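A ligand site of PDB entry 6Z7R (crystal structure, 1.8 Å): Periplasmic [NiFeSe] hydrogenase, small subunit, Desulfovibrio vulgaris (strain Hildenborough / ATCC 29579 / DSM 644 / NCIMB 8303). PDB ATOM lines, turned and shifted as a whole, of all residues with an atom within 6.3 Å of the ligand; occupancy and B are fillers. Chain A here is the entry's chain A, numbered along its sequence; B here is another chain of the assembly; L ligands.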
ATOM      1  N   GLY A 158     -24.517 -29.174  17.801  1.00  0.00           N
ATOM      2  CA  GLY A 158     -24.311 -27.853  18.379  1.00  0.00           C
ATOM      3  C   GLY A 158     -22.842 -27.525  18.293  1.00  0.00           C
ATOM      4  O   GLY A 158     -22.032 -28.455  18.213  1.00  0.00           O
ATOM      5  N   CYS A 159     -22.477 -26.239  18.267  1.00  0.00           N
ATOM      6  CA  CYS A 159     -21.078 -25.806  18.189  1.00  0.00           C
ATOM      7  C   CYS A 159     -20.925 -24.620  19.099  1.00  0.00           C
ATOM      8  O   CYS A 159     -20.814 -23.464  18.653  1.00  0.00           O
ATOM      9  CB  CYS A 159     -20.679 -25.457  16.754  1.00  0.00           C
ATOM     10  SG  CYS A 159     -18.942 -25.288  16.466  1.00  0.00           S
ATOM     11  N   PRO A 160     -20.966 -24.849  20.405  1.00  0.00           N
ATOM     12  CA  PRO A 160     -21.179 -26.132  21.072  1.00  0.00           C
ATOM     13  C   PRO A 160     -22.644 -26.476  21.308  1.00  0.00           C
ATOM     14  O   PRO A 160     -23.494 -25.608  21.158  1.00  0.00           O
ATOM     15  CB  PRO A 160     -20.477 -25.922  22.395  1.00  0.00           C
ATOM     16  CG  PRO A 160     -20.742 -24.463  22.688  1.00  0.00           C
ATOM     17  CD  PRO A 160     -20.872 -23.747  21.380  1.00  0.00           C
ATOM     18  N   TRP A 165     -28.595 -30.300  26.481  1.00  0.00           N
ATOM     19  CA  TRP A 165     -28.703 -31.342  25.457  1.00  0.00           C
ATOM     20  C   TRP A 165     -27.811 -32.535  25.761  1.00  0.00           C
ATOM     21  O   TRP A 165     -28.205 -33.679  25.535  1.00  0.00           O
ATOM     22  CB  TRP A 165     -28.372 -30.781  24.080  1.00  0.00           C
ATOM     23  CG  TRP A 165     -29.174 -29.572  23.648  1.00  0.00           C
ATOM     24  CD1 TRP A 165     -30.357 -29.137  24.161  1.00  0.00           C
ATOM     25  CD2 TRP A 165     -28.832 -28.661  22.596  1.00  0.00           C
ATOM     26  NE1 TRP A 165     -30.765 -27.997  23.502  1.00  0.00           N
ATOM     27  CE2 TRP A 165     -29.860 -27.707  22.526  1.00  0.00           C
ATOM     28  CE3 TRP A 165     -27.777 -28.592  21.693  1.00  0.00           C
ATOM     29  CZ2 TRP A 165     -29.844 -26.665  21.612  1.00  0.00           C
ATOM     30  CZ3 TRP A 165     -27.763 -27.538  20.772  1.00  0.00           C
ATOM     31  CH2 TRP A 165     -28.802 -26.593  20.743  1.00  0.00           C
ATOM     32  N   ILE A 207     -36.361 -23.479  14.952  1.00  0.00           N
ATOM     33  CA  ILE A 207     -36.161 -22.192  15.610  1.00  0.00           C
ATOM     34  C   ILE A 207     -37.149 -21.158  15.079  1.00  0.00           C
ATOM     35  O   ILE A 207     -37.815 -20.461  15.852  1.00  0.00           O
ATOM     36  CB  ILE A 207     -34.719 -21.675  15.444  1.00  0.00           C
ATOM     37  CG1 ILE A 207     -33.734 -22.545  16.203  1.00  0.00           C
ATOM     38  CG2 ILE A 207     -34.610 -20.213  15.903  1.00  0.00           C
ATOM     39  CD1 ILE A 207     -33.627 -22.168  17.719  1.00  0.00           C
ATOM     40  N   GLY A 240     -32.352 -19.278  11.686  1.00  0.00           N
ATOM     41  CA  GLY A 240     -33.500 -19.913  12.282  1.00  0.00           C
ATOM     42  C   GLY A 240     -34.358 -20.684  11.286  1.00  0.00           C
ATOM     43  O   GLY A 240     -34.690 -21.847  11.506  1.00  0.00           O
ATOM     44  N   THR A 243     -33.050 -24.243  10.876  1.00  0.00           N
ATOM     45  CA  THR A 243     -32.387 -24.797  12.048  1.00  0.00           C
ATOM     46  C   THR A 243     -33.347 -25.350  13.082  1.00  0.00           C
ATOM     47  O   THR A 243     -34.233 -24.637  13.569  1.00  0.00           O
ATOM     48  CB  THR A 243     -31.540 -23.704  12.716  1.00  0.00           C
ATOM     49  OG1 THR A 243     -30.668 -23.155  11.733  1.00  0.00           O
ATOM     50  CG2 THR A 243     -30.728 -24.296  13.838  1.00  0.00           C
ATOM     51  N   MET A 244     -33.068 -26.606  13.510  1.00  0.00           N
ATOM     52  CA  MET A 244     -33.897 -27.386  14.434  1.00  0.00           C
ATOM     53  C   MET A 244     -33.163 -27.477  15.789  1.00  0.00           C
ATOM     54  O   MET A 244     -32.291 -28.328  15.975  1.00  0.00           O
ATOM     55  CB  MET A 244     -34.143 -28.794  13.899  1.00  0.00           C
ATOM     56  CG  MET A 244     -34.639 -28.914  12.481  1.00  0.00           C
ATOM     57  SD  MET A 244     -36.298 -28.275  12.303  1.00  0.00           S
ATOM     58  CE  MET A 244     -37.233 -29.311  13.388  1.00  0.00           C
ATOM     59  N   ALA A 245     -33.547 -26.603  16.716  1.00  0.00           N
ATOM     60  CA  ALA A 245     -32.992 -26.584  18.066  1.00  0.00           C
ATOM     61  C   ALA A 245     -33.943 -25.780  18.933  1.00  0.00           C
ATOM     62  O   ALA A 245     -34.798 -25.074  18.425  1.00  0.00           O
ATOM     63  CB  ALA A 245     -31.585 -25.967  18.098  1.00  0.00           C
ATOM     64  N   ASP A 246     -33.786 -25.885  20.252  1.00  0.00           N
ATOM     65  CA  ASP A 246     -34.723 -25.293  21.190  1.00  0.00           C
ATOM     66  C   ASP A 246     -34.157 -24.118  21.991  1.00  0.00           C
ATOM     67  O   ASP A 246     -34.603 -23.853  23.119  1.00  0.00           O
ATOM     68  CB  ASP A 246     -35.267 -26.374  22.129  1.00  0.00           C
ATOM     69  CG  ASP A 246     -34.171 -27.033  22.979  1.00  0.00           C
ATOM     70  OD1 ASP A 246     -33.070 -26.474  23.148  1.00  0.00           O
ATOM     71  OD2 ASP A 246     -34.430 -28.140  23.492  1.00  0.00           O
ATOM     72  N   CYS A 247     -33.168 -23.410  21.436  1.00  0.00           N
ATOM     73  CA  CYS A 247     -32.527 -22.336  22.192  1.00  0.00           C
ATOM     74  C   CYS A 247     -33.497 -21.185  22.446  1.00  0.00           C
ATOM     75  O   CYS A 247     -33.295 -20.417  23.400  1.00  0.00           O
ATOM     76  CB  CYS A 247     -31.311 -21.802  21.445  1.00  0.00           C
ATOM     77  SG  CYS A 247     -30.256 -23.047  20.671  1.00  0.00           S
ATOM     78  N   PHE A 248     -34.506 -21.047  21.586  1.00  0.00           N
ATOM     79  CA  PHE A 248     -35.545 -20.026  21.722  1.00  0.00           C
ATOM     80  C   PHE A 248     -36.257 -20.084  23.067  1.00  0.00           C
ATOM     81  O   PHE A 248     -36.710 -19.053  23.583  1.00  0.00           O
ATOM     82  CB  PHE A 248     -36.595 -20.147  20.611  1.00  0.00           C
ATOM     83  CG  PHE A 248     -37.233 -21.513  20.506  1.00  0.00           C
ATOM     84  CD1 PHE A 248     -38.136 -21.953  21.469  1.00  0.00           C
ATOM     85  CD2 PHE A 248     -37.063 -22.296  19.375  1.00  0.00           C
ATOM     86  CE1 PHE A 248     -38.748 -23.194  21.357  1.00  0.00           C
ATOM     87  CE2 PHE A 248     -37.699 -23.532  19.236  1.00  0.00           C
ATOM     88  CZ  PHE A 248     -38.542 -23.981  20.227  1.00  0.00           C
ATOM     89  N   TRP A 252     -29.429 -19.706  26.781  1.00  0.00           N
ATOM     90  CA  TRP A 252     -28.048 -20.117  26.989  1.00  0.00           C
ATOM     91  C   TRP A 252     -27.499 -19.519  28.252  1.00  0.00           C
ATOM     92  O   TRP A 252     -27.939 -18.447  28.683  1.00  0.00           O
ATOM     93  CB  TRP A 252     -27.142 -19.711  25.835  1.00  0.00           C
ATOM     94  CG  TRP A 252     -27.166 -20.707  24.747  1.00  0.00           C
ATOM     95  CD1 TRP A 252     -28.130 -20.868  23.800  1.00  0.00           C
ATOM     96  CD2 TRP A 252     -26.197 -21.716  24.522  1.00  0.00           C
ATOM     97  NE1 TRP A 252     -27.804 -21.927  22.976  1.00  0.00           N
ATOM     98  CE2 TRP A 252     -26.632 -22.472  23.401  1.00  0.00           C
ATOM     99  CE3 TRP A 252     -25.018 -22.076  25.151  1.00  0.00           C
ATOM    100  CZ2 TRP A 252     -25.919 -23.543  22.905  1.00  0.00           C
ATOM    101  CZ3 TRP A 252     -24.318 -23.155  24.671  1.00  0.00           C
ATOM    102  CH2 TRP A 252     -24.761 -23.883  23.557  1.00  0.00           C
ATOM    103  N   TRP A 258     -29.429 -15.445  24.282  1.00  0.00           N
ATOM    104  CA  TRP A 258     -29.306 -16.458  23.247  1.00  0.00           C
ATOM    105  C   TRP A 258     -28.993 -15.781  21.928  1.00  0.00           C
ATOM    106  O   TRP A 258     -29.029 -14.551  21.805  1.00  0.00           O
ATOM    107  CB  TRP A 258     -30.551 -17.353  23.195  1.00  0.00           C
ATOM    108  CG  TRP A 258     -31.789 -16.724  22.731  1.00  0.00           C
ATOM    109  CD1 TRP A 258     -32.442 -15.690  23.331  1.00  0.00           C
ATOM    110  CD2 TRP A 258     -32.594 -17.099  21.595  1.00  0.00           C
ATOM    111  NE1 TRP A 258     -33.573 -15.384  22.618  1.00  0.00           N
ATOM    112  CE2 TRP A 258     -33.691 -16.239  21.561  1.00  0.00           C
ATOM    113  CE3 TRP A 258     -32.476 -18.097  20.598  1.00  0.00           C
ATOM    114  CZ2 TRP A 258     -34.684 -16.335  20.575  1.00  0.00           C
ATOM    115  CZ3 TRP A 258     -33.447 -18.188  19.631  1.00  0.00           C
ATOM    116  CH2 TRP A 258     -34.535 -17.317  19.626  1.00  0.00           C
ATOM    117  N   CYS A 259     -28.704 -16.616  20.920  1.00  0.00           N
ATOM    118  CA  CYS A 259     -28.037 -16.106  19.708  1.00  0.00           C
ATOM    119  C   CYS A 259     -28.937 -15.176  18.909  1.00  0.00           C
ATOM    120  O   CYS A 259     -28.479 -14.117  18.456  1.00  0.00           O
ATOM    121  CB  CYS A 259     -27.578 -17.281  18.835  1.00  0.00           C
ATOM    122  SG  CYS A 259     -26.525 -18.512  19.780  1.00  0.00           S
ATOM    123  N   VAL A 260     -30.224 -15.516  18.750  1.00  0.00           N
ATOM    124  CA  VAL A 260     -31.163 -14.624  18.047  1.00  0.00           C
ATOM    125  C   VAL A 260     -31.373 -13.301  18.787  1.00  0.00           C
ATOM    126  O   VAL A 260     -31.545 -12.245  18.163  1.00  0.00           O
ATOM    127  CB  VAL A 260     -32.516 -15.315  17.789  1.00  0.00           C
ATOM    128  CG1 VAL A 260     -33.505 -14.335  17.197  1.00  0.00           C
ATOM    129  CG2 VAL A 260     -32.388 -16.436  16.809  1.00  0.00           C
ATOM    130  N   VAL A 264     -27.473 -13.236  15.679  1.00  0.00           N
ATOM    131  CA  VAL A 264     -28.221 -14.080  14.760  1.00  0.00           C
ATOM    132  C   VAL A 264     -28.007 -15.536  15.159  1.00  0.00           C
ATOM    133  O   VAL A 264     -27.067 -15.859  15.865  1.00  0.00           O
ATOM    134  CB  VAL A 264     -27.776 -13.877  13.308  1.00  0.00           C
ATOM    135  CG1 VAL A 264     -28.142 -12.461  12.831  1.00  0.00           C
ATOM    136  CG2 VAL A 264     -26.282 -14.129  13.168  1.00  0.00           C
ATOM    137  N   CYS A 265     -28.891 -16.408  14.708  1.00  0.00           N
ATOM    138  CA  CYS A 265     -28.601 -17.826  14.707  1.00  0.00           C
ATOM    139  C   CYS A 265     -27.716 -18.154  13.501  1.00  0.00           C
ATOM    140  O   CYS A 265     -28.062 -17.825  12.366  1.00  0.00           O
ATOM    141  CB  CYS A 265     -29.913 -18.608  14.633  1.00  0.00           C
ATOM    142  SG  CYS A 265     -29.804 -20.424  14.576  1.00  0.00           S
ATOM    143  N   ILE A 266     -26.616 -18.876  13.731  1.00  0.00           N
ATOM    144  CA  ILE A 266     -25.779 -19.325  12.624  1.00  0.00           C
ATOM    145  C   ILE A 266     -26.012 -20.810  12.301  1.00  0.00           C
ATOM    146  O   ILE A 266     -25.263 -21.396  11.516  1.00  0.00           O
ATOM    147  CB  ILE A 266     -24.290 -19.019  12.893  1.00  0.00           C
ATOM    148  CG1 ILE A 266     -23.751 -19.781  14.102  1.00  0.00           C
ATOM    149  CG2 ILE A 266     -24.102 -17.540  13.092  1.00  0.00           C
ATOM    150  CD1 ILE A 266     -22.164 -19.697  14.317  1.00  0.00           C
ATOM    151  N   GLY A 267     -27.026 -21.424  12.892  1.00  0.00           N
ATOM    152  CA  GLY A 267     -27.436 -22.802  12.588  1.00  0.00           C
ATOM    153  C   GLY A 267     -26.467 -23.903  12.986  1.00  0.00           C
ATOM    154  O   GLY A 267     -26.338 -24.896  12.255  1.00  0.00           O
ATOM    155  N   CYS A 268     -25.858 -23.795  14.174  1.00  0.00           N
ATOM    156  CA  CYS A 268     -24.668 -24.587  14.504  1.00  0.00           C
ATOM    157  C   CYS A 268     -24.982 -26.058  14.749  1.00  0.00           C
ATOM    158  O   CYS A 268     -24.054 -26.870  14.770  1.00  0.00           O
ATOM    159  CB  CYS A 268     -23.963 -23.945  15.713  1.00  0.00           C
ATOM    160  SG  CYS A 268     -24.853 -24.114  17.237  1.00  0.00           S
ATOM    161  N   VAL A 269     -26.271 -26.399  14.873  1.00  0.00           N
ATOM    162  CA  VAL A 269     -26.713 -27.769  15.130  1.00  0.00           C
ATOM    163  C   VAL A 269     -26.932 -28.594  13.870  1.00  0.00           C
ATOM    164  O   VAL A 269     -27.170 -29.811  13.957  1.00  0.00           O
ATOM    165  CB  VAL A 269     -28.036 -27.763  15.935  1.00  0.00           C
ATOM    166  CG1 VAL A 269     -27.889 -27.058  17.353  1.00  0.00           C
ATOM    167  CG2 VAL A 269     -29.118 -27.049  15.144  1.00  0.00           C
ATOM    168  N   ARG B  62     -13.803 -21.336  16.993  1.00  0.00           N
ATOM    169  CA  ARG B  62     -13.802 -22.780  16.991  1.00  0.00           C
ATOM    170  C   ARG B  62     -12.401 -23.345  16.918  1.00  0.00           C
ATOM    171  O   ARG B  62     -12.250 -24.561  16.877  1.00  0.00           O
ATOM    172  CB  ARG B  62     -14.626 -23.338  15.804  1.00  0.00           C
ATOM    173  CG  ARG B  62     -16.118 -23.434  16.123  1.00  0.00           C
ATOM    174  CD  ARG B  62     -16.811 -22.097  16.056  1.00  0.00           C
ATOM    175  NE  ARG B  62     -18.213 -22.186  16.450  1.00  0.00           N
ATOM    176  CZ  ARG B  62     -19.003 -21.161  16.707  1.00  0.00           C
ATOM    177  NH1 ARG B  62     -18.570 -19.928  16.582  1.00  0.00           N
ATOM    178  NH2 ARG B  62     -20.284 -21.373  17.068  1.00  0.00           N
ATOM    179  N   ARG B 171     -23.888 -16.128  24.028  1.00  0.00           N
ATOM    180  CA  ARG B 171     -23.692 -17.442  24.622  1.00  0.00           C
ATOM    181  C   ARG B 171     -22.193 -17.651  24.797  1.00  0.00           C
ATOM    182  O   ARG B 171     -21.376 -16.882  24.290  1.00  0.00           O
ATOM    183  CB  ARG B 171     -24.304 -18.540  23.751  1.00  0.00           C
ATOM    184  CG  ARG B 171     -23.580 -18.804  22.451  1.00  0.00           C
ATOM    185  CD  ARG B 171     -23.880 -20.179  21.884  1.00  0.00           C
ATOM    186  NE  ARG B 171     -23.535 -20.224  20.470  1.00  0.00           N
ATOM    187  CZ  ARG B 171     -23.467 -21.343  19.760  1.00  0.00           C
ATOM    188  NH1 ARG B 171     -23.696 -22.505  20.330  1.00  0.00           N
ATOM    189  NH2 ARG B 171     -23.153 -21.307  18.496  1.00  0.00           N
ATOM    190  N   GLN B 176     -21.709 -14.757  20.061  1.00  0.00           N
ATOM    191  CA  GLN B 176     -22.258 -14.119  18.882  1.00  0.00           C
ATOM    192  C   GLN B 176     -22.089 -12.609  18.933  1.00  0.00           C
ATOM    193  O   GLN B 176     -22.231 -11.952  17.897  1.00  0.00           O
ATOM    194  CB  GLN B 176     -23.741 -14.458  18.762  1.00  0.00           C
ATOM    195  CG  GLN B 176     -24.024 -15.898  18.671  1.00  0.00           C
ATOM    196  CD  GLN B 176     -23.798 -16.417  17.293  1.00  0.00           C
ATOM    197  OE1 GLN B 176     -23.249 -15.725  16.429  1.00  0.00           O
ATOM    198  NE2 GLN B 176     -24.168 -17.670  17.076  1.00  0.00           N
HETATM  199 FE1  LIG L   1     -26.756 -22.803  17.427  1.00  0.00          FE
HETATM  200 FE2  LIG L   1     -28.760 -21.197  16.391  1.00  0.00          FE
HETATM  201 FE3  LIG L   1     -27.254 -20.268  18.472  1.00  0.00          FE
HETATM  202 FE4  LIG L   1     -29.117 -22.334  18.817  1.00  0.00          FE
HETATM  203  S1  LIG L   1     -29.494 -20.182  18.250  1.00  0.00           S
HETATM  204  S2  LIG L   1     -26.961 -22.223  19.577  1.00  0.00           S
HETATM  205  S3  LIG L   1     -28.917 -23.436  16.848  1.00  0.00           S
HETATM  206  S4  LIG L   1     -26.465 -20.811  16.378  1.00  0.00           S
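FE2 of the ligand is bound by SG of Cys 265.
S4 of the ligand lies close to N of Gly 267, at 3.6 Å.
SG of Cys 247 is bound to FE4 of the ligand (2.3 Å).
S4 of the ligand lies close to N of Cys 268 (3.8 Å).
S2 of the ligand sits close to NH1 of Arg 171 of chain B, 3.4 Å away.
SG of Cys 268 is bound to FE1 of the ligand.
The backbone NH of Ile 266 lies close to a sulfur (S4) of the ligand (3.3 Å).
NE1 of Trp 252 sits close to S2 of the ligand.
An iron atom (FE3) of the ligand is bound by the side-chain sulfur of Cys 259, at 2.3 Å.
The backbone carbonyl oxygen (O) of Cys 159 is in hydrogen-bond range of the guanidinium group (NH2) of Arg 171 of chain B.
O of Cys 259 sits at hydrogen-bond distance from N of Val 264 (3.1 Å).
The side-chain sulfur (SG) of Cys 247 sits close to the indole nitrogen (NE1) of Trp 252, 3.5 Å away.
The side-chain sulfur (SG) of Cys 268 sits close to the guanidinium group (NH2) of Arg 171 of chain B (3.5 Å).
O of Thr 243 is in hydrogen-bond range of N of Ile 207 (2.8 Å).
The backbone NH (N) of Gly 267 sits close to the side-chain sulfur (SG) of Cys 265, 3.4 Å away.
The side-chain sulfur (SG) of Cys 259 lies close to the side-chain amide nitrogen (NE2) of Gln 176 of chain B (3.7 Å).
The side-chain sulfur (SG) of Cys 268 lies close to the backbone NH (N) of Cys 159, at 3.3 Å.
Merely in contact with the ligand: Thr 243 (3.6 Å), Ala 245 (3.9 Å), Val 269 (3.8 Å) and Gln 176 of chain B (3.95 Å).
Within 4 Å of the ligand: Thr 243, Ala 245, Cys 247, Trp 252, Cys 259, Cys 265, Ile 266, Gly 267, Cys 268, Val 269, Arg 171 of chain B and Gln 176 of chain B.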
